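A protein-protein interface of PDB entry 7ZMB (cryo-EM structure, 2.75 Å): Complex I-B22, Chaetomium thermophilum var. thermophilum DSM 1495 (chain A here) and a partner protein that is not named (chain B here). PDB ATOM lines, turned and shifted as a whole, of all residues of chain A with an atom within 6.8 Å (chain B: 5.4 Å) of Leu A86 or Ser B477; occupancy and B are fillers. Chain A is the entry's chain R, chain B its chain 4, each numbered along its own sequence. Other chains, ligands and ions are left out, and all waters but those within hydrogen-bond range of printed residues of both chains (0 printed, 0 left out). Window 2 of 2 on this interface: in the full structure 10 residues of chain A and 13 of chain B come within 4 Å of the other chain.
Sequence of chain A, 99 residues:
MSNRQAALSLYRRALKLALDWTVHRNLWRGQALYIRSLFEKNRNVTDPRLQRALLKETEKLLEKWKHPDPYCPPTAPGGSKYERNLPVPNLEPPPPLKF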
ATOM      1  N   TYR A  82     -34.480  -4.259 -16.212  1.00  0.00           N
ATOM      2  CA  TYR A  82     -33.155  -3.665 -16.084  1.00  0.00           C
ATOM      3  C   TYR A  82     -32.247  -4.521 -15.212  1.00  0.00           C
ATOM      4  O   TYR A  82     -32.657  -5.013 -14.162  1.00  0.00           O
ATOM      5  CB  TYR A  82     -33.261  -2.270 -15.483  1.00  0.00           C
ATOM      6  CG  TYR A  82     -31.933  -1.573 -15.343  1.00  0.00           C
ATOM      7  CD1 TYR A  82     -31.115  -1.370 -16.442  1.00  0.00           C
ATOM      8  CD2 TYR A  82     -31.487  -1.136 -14.106  1.00  0.00           C
ATOM      9  CE1 TYR A  82     -29.897  -0.738 -16.318  1.00  0.00           C
ATOM     10  CE2 TYR A  82     -30.265  -0.505 -13.968  1.00  0.00           C
ATOM     11  CZ  TYR A  82     -29.475  -0.308 -15.079  1.00  0.00           C
ATOM     12  OH  TYR A  82     -28.259   0.322 -14.954  1.00  0.00           O
ATOM     13  N   GLU A  83     -30.999  -4.685 -15.658  1.00  0.00           N
ATOM     14  CA  GLU A  83     -29.957  -5.477 -15.000  1.00  0.00           C
ATOM     15  C   GLU A  83     -30.471  -6.816 -14.479  1.00  0.00           C
ATOM     16  O   GLU A  83     -30.093  -7.243 -13.388  1.00  0.00           O
ATOM     17  CB  GLU A  83     -29.280  -4.670 -13.873  1.00  0.00           C
ATOM     18  CG  GLU A  83     -30.161  -4.221 -12.713  1.00  0.00           C
ATOM     19  CD  GLU A  83     -29.393  -3.477 -11.639  1.00  0.00           C
ATOM     20  OE1 GLU A  83     -28.197  -3.189 -11.853  1.00  0.00           O
ATOM     21  OE2 GLU A  83     -29.981  -3.188 -10.579  1.00  0.00           O
ATOM     22  N   ARG A  84     -31.287  -7.509 -15.279  1.00  0.00           N
ATOM     23  CA  ARG A  84     -31.912  -8.756 -14.845  1.00  0.00           C
ATOM     24  C   ARG A  84     -30.972  -9.949 -14.974  1.00  0.00           C
ATOM     25  O   ARG A  84     -30.682 -10.634 -13.987  1.00  0.00           O
ATOM     26  CB  ARG A  84     -33.183  -9.017 -15.651  1.00  0.00           C
ATOM     27  CG  ARG A  84     -33.674 -10.451 -15.547  1.00  0.00           C
ATOM     28  CD  ARG A  84     -34.996 -10.639 -16.237  1.00  0.00           C
ATOM     29  NE  ARG A  84     -36.095 -10.119 -15.437  1.00  0.00           N
ATOM     30  CZ  ARG A  84     -37.352 -10.055 -15.854  1.00  0.00           C
ATOM     31  NH1 ARG A  84     -37.670 -10.474 -17.067  1.00  0.00           N
ATOM     32  NH2 ARG A  84     -38.289  -9.567 -15.059  1.00  0.00           N
ATOM     33  N   ASN A  85     -30.512 -10.231 -16.190  1.00  0.00           N
ATOM     34  CA  ASN A  85     -29.647 -11.371 -16.476  1.00  0.00           C
ATOM     35  C   ASN A  85     -28.307 -10.805 -16.926  1.00  0.00           C
ATOM     36  O   ASN A  85     -28.055 -10.643 -18.121  1.00  0.00           O
ATOM     37  CB  ASN A  85     -30.261 -12.274 -17.534  1.00  0.00           C
ATOM     38  CG  ASN A  85     -31.590 -12.854 -17.104  1.00  0.00           C
ATOM     39  OD1 ASN A  85     -31.779 -13.195 -15.938  1.00  0.00           O
ATOM     40  ND2 ASN A  85     -32.520 -12.964 -18.042  1.00  0.00           N
ATOM     41  N   LEU A  86     -27.464 -10.510 -15.979  1.00  0.00           N
ATOM     42  CA  LEU A  86     -26.236  -9.808 -16.305  1.00  0.00           C
ATOM     43  C   LEU A  86     -25.106 -10.797 -16.548  1.00  0.00           C
ATOM     44  O   LEU A  86     -24.846 -11.650 -15.691  1.00  0.00           O
ATOM     45  CB  LEU A  86     -25.854  -8.854 -15.187  1.00  0.00           C
ATOM     46  CG  LEU A  86     -26.792  -7.665 -15.015  1.00  0.00           C
ATOM     47  CD1 LEU A  86     -26.294  -6.742 -13.913  1.00  0.00           C
ATOM     48  CD2 LEU A  86     -26.926  -6.916 -16.328  1.00  0.00           C
ATOM     49  N   PRO A  87     -24.427 -10.722 -17.687  1.00  0.00           N
ATOM     50  CA  PRO A  87     -23.237 -11.550 -17.889  1.00  0.00           C
ATOM     51  C   PRO A  87     -22.114 -11.099 -16.973  1.00  0.00           C
ATOM     52  O   PRO A  87     -22.074  -9.962 -16.507  1.00  0.00           O
ATOM     53  CB  PRO A  87     -22.884 -11.314 -19.360  1.00  0.00           C
ATOM     54  CG  PRO A  87     -23.428  -9.966 -19.654  1.00  0.00           C
ATOM     55  CD  PRO A  87     -24.671  -9.815 -18.821  1.00  0.00           C
ATOM     56  N   VAL A  88     -21.197 -12.016 -16.707  1.00  0.00           N
ATOM     57  CA  VAL A  88     -20.067 -11.653 -15.848  1.00  0.00           C
ATOM     58  C   VAL A  88     -19.193 -10.643 -16.581  1.00  0.00           C
ATOM     59  O   VAL A  88     -18.976 -10.778 -17.799  1.00  0.00           O
ATOM     60  CB  VAL A  88     -19.274 -12.897 -15.444  1.00  0.00           C
ATOM     61  CG1 VAL A  88     -20.215 -13.975 -14.935  1.00  0.00           C
ATOM     62  CG2 VAL A  88     -18.404 -13.393 -16.576  1.00  0.00           C
ATOM     63  N   PRO A  89     -18.734  -9.588 -15.917  1.00  0.00           N
ATOM     64  CA  PRO A  89     -17.915  -8.586 -16.617  1.00  0.00           C
ATOM     65  C   PRO A  89     -16.603  -9.131 -17.153  1.00  0.00           C
ATOM     66  O   PRO A  89     -16.036  -8.544 -18.083  1.00  0.00           O
ATOM     67  CB  PRO A  89     -17.685  -7.517 -15.541  1.00  0.00           C
ATOM     68  CG  PRO A  89     -18.845  -7.676 -14.611  1.00  0.00           C
ATOM     69  CD  PRO A  89     -19.150  -9.138 -14.583  1.00  0.00           C
ATOM     70  N   ARG B 404     -19.041  -7.734  -4.336  1.00  0.00           N
ATOM     71  CA  ARG B 404     -20.366  -7.611  -4.911  1.00  0.00           C
ATOM     72  C   ARG B 404     -20.543  -8.750  -5.901  1.00  0.00           C
ATOM     73  O   ARG B 404     -19.626  -9.063  -6.663  1.00  0.00           O
ATOM     74  CB  ARG B 404     -20.541  -6.242  -5.584  1.00  0.00           C
ATOM     75  CG  ARG B 404     -21.872  -5.994  -6.260  1.00  0.00           C
ATOM     76  CD  ARG B 404     -21.853  -6.434  -7.707  1.00  0.00           C
ATOM     77  NE  ARG B 404     -20.886  -5.703  -8.515  1.00  0.00           N
ATOM     78  CZ  ARG B 404     -20.896  -4.390  -8.724  1.00  0.00           C
ATOM     79  NH1 ARG B 404     -21.844  -3.623  -8.213  1.00  0.00           N
ATOM     80  NH2 ARG B 404     -19.955  -3.845  -9.478  1.00  0.00           N
ATOM     81  N   GLY B 405     -21.723  -9.362  -5.874  1.00  0.00           N
ATOM     82  CA  GLY B 405     -22.066 -10.434  -6.786  1.00  0.00           C
ATOM     83  C   GLY B 405     -21.009 -11.497  -7.014  1.00  0.00           C
ATOM     84  O   GLY B 405     -20.566 -11.692  -8.144  1.00  0.00           O
ATOM     85  N   LEU B 406     -20.577 -12.190  -5.965  1.00  0.00           N
ATOM     86  CA  LEU B 406     -19.674 -13.310  -6.170  1.00  0.00           C
ATOM     87  C   LEU B 406     -20.386 -14.584  -6.574  1.00  0.00           C
ATOM     88  O   LEU B 406     -19.727 -15.524  -7.029  1.00  0.00           O
ATOM     89  CB  LEU B 406     -18.832 -13.584  -4.923  1.00  0.00           C
ATOM     90  CG  LEU B 406     -17.800 -12.532  -4.566  1.00  0.00           C
ATOM     91  CD1 LEU B 406     -17.129 -12.881  -3.266  1.00  0.00           C
ATOM     92  CD2 LEU B 406     -16.788 -12.460  -5.676  1.00  0.00           C
ATOM     93  N   GLN B 408     -21.979 -15.080  -9.130  1.00  0.00           N
ATOM     94  CA  GLN B 408     -21.765 -15.328 -10.548  1.00  0.00           C
ATOM     95  C   GLN B 408     -20.514 -16.141 -10.827  1.00  0.00           C
ATOM     96  O   GLN B 408     -20.399 -16.716 -11.911  1.00  0.00           O
ATOM     97  CB  GLN B 408     -21.686 -14.024 -11.338  1.00  0.00           C
ATOM     98  CG  GLN B 408     -22.988 -13.311 -11.528  1.00  0.00           C
ATOM     99  CD  GLN B 408     -22.925 -12.349 -12.678  1.00  0.00           C
ATOM    100  OE1 GLN B 408     -21.907 -11.705 -12.903  1.00  0.00           O
ATOM    101  NE2 GLN B 408     -24.015 -12.251 -13.426  1.00  0.00           N
ATOM    102  N   GLY B 475     -26.305  -8.739  -5.298  1.00  0.00           N
ATOM    103  CA  GLY B 475     -26.250  -7.295  -5.364  1.00  0.00           C
ATOM    104  C   GLY B 475     -25.602  -6.758  -6.614  1.00  0.00           C
ATOM    105  O   GLY B 475     -25.062  -5.646  -6.602  1.00  0.00           O
ATOM    106  N   GLY B 476     -25.642  -7.517  -7.699  1.00  0.00           N
ATOM    107  CA  GLY B 476     -24.962  -7.120  -8.910  1.00  0.00           C
ATOM    108  C   GLY B 476     -24.214  -8.261  -9.551  1.00  0.00           C
ATOM    109  O   GLY B 476     -24.272  -9.392  -9.071  1.00  0.00           O
ATOM    110  N   SER B 477     -23.500  -7.978 -10.638  1.00  0.00           N
ATOM    111  CA  SER B 477     -22.905  -9.055 -11.425  1.00  0.00           C
ATOM    112  C   SER B 477     -21.624  -9.573 -10.778  1.00  0.00           C
ATOM    113  O   SER B 477     -21.585 -10.700 -10.284  1.00  0.00           O
ATOM    114  CB  SER B 477     -22.651  -8.565 -12.855  1.00  0.00           C
ATOM    115  OG  SER B 477     -21.703  -7.516 -12.874  1.00  0.00           O
ATOM    116  N   VAL B 478     -20.578  -8.751 -10.745  1.00  0.00           N
ATOM    117  CA  VAL B 478     -19.408  -8.976  -9.903  1.00  0.00           C
ATOM    118  C   VAL B 478     -18.868  -7.597  -9.591  1.00  0.00           C
ATOM    119  O   VAL B 478     -19.130  -6.630 -10.313  1.00  0.00           O
ATOM    120  CB  VAL B 478     -18.255  -9.816 -10.515  1.00  0.00           C
ATOM    121  CG1 VAL B 478     -18.708 -11.191 -11.003  1.00  0.00           C
ATOM    122  CG2 VAL B 478     -17.508  -9.032 -11.571  1.00  0.00           C
ATOM    123  N   SER B 479     -18.120  -7.497  -8.504  1.00  0.00           N
ATOM    124  CA  SER B 479     -17.474  -6.235  -8.206  1.00  0.00           C
ATOM    125  C   SER B 479     -16.496  -5.892  -9.325  1.00  0.00           C
ATOM    126  O   SER B 479     -15.697  -6.728  -9.749  1.00  0.00           O
ATOM    127  CB  SER B 479     -16.765  -6.317  -6.859  1.00  0.00           C
ATOM    128  OG  SER B 479     -16.089  -5.117  -6.558  1.00  0.00           O
ATOM    129  N   LEU B 480     -16.577  -4.662  -9.815  1.00  0.00           N
ATOM    130  CA  LEU B 480     -15.745  -4.232 -10.925  1.00  0.00           C
ATOM    131  C   LEU B 480     -14.336  -3.862 -10.503  1.00  0.00           C
ATOM    132  O   LEU B 480     -13.520  -3.521 -11.364  1.00  0.00           O
ATOM    133  CB  LEU B 480     -16.395  -3.053 -11.655  1.00  0.00           C
ATOM    134  CG  LEU B 480     -17.804  -3.332 -12.171  1.00  0.00           C
ATOM    135  CD1 LEU B 480     -18.362  -2.113 -12.855  1.00  0.00           C
ATOM    136  CD2 LEU B 480     -17.795  -4.519 -13.116  1.00  0.00           C
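The backbone carbonyl oxygen of Leu A86 is in hydrogen-bond range of the side-chain amide nitrogen of Gln B408, 2.5 Å away.
The guanidinium group (NE) of Arg B404 is in hydrogen-bond range of the backbone carbonyl oxygen (O) of Val B478.
The backbone carbonyl oxygen (O) of Gly B405 lies close to the backbone carbonyl oxygen (O) of Ser B477 (2.6 Å).
O of Ser B477 sits close to OE1 of Gln B408, 2.8 Å away.
CB of Leu A86 touches CB of Ser B477, at 3.97 Å.
O of Pro A87 touches CB of Ser B477, at 3.95 Å.
Gln B408 touches Val A88.
Pro A89 touches Ser B477.
CG2 of Val B478 touches CD of Pro A89 (3.4 Å).
CD2 of Leu B480 touches CG of Pro A89, at 3.6 Å.
Leu A86 touches just these residues of chain B: Gln B408 (2.5 Å) and Ser B477 (3.97 Å).
Ser B477 touches just these residues of chain A: Leu A86 (3.97 Å), Pro A87 (3.95 Å) and Pro A89 (3.3 Å).
Printed residues of chain A within 4 Å of Val B478: Pro A89.
Of the printed residues of chain A, Gln B408 touches Leu A86 (2.5 Å) and Val A88 (3.5 Å).
Printed residues of chain B within 4 Å of Pro A89: Ser B477, Val B478 and Leu B480.
Of the printed residues of chain A, Leu B480 touches Pro A89.
Gly B476 touches none of the printed residues of chain A.
The nearest residue of chain A that does not touch Ser B477 is Val A88 (5.0 Å).
The nearest printed residue of chain B that does not touch Pro A89 is Gln B408 (4.1 Å).
Of the 8 printed residues of chain A, 4 touch a printed residue of chain B.
Of the 10 printed residues of chain B, 4 touch a printed residue of chain A.
Printed residues of chain B that touch a printed residue of chain A: Gln B408, Ser B477, Val B478 and Leu B480.
Hydrophobic or aromatic side chains of chain B that line the printed part of chain A: Val B478 and Leu B480.
Among the printed residues, no Asp or Glu carboxylate lies within 4 Å of a Lys or Arg side-chain nitrogen of the other chain.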
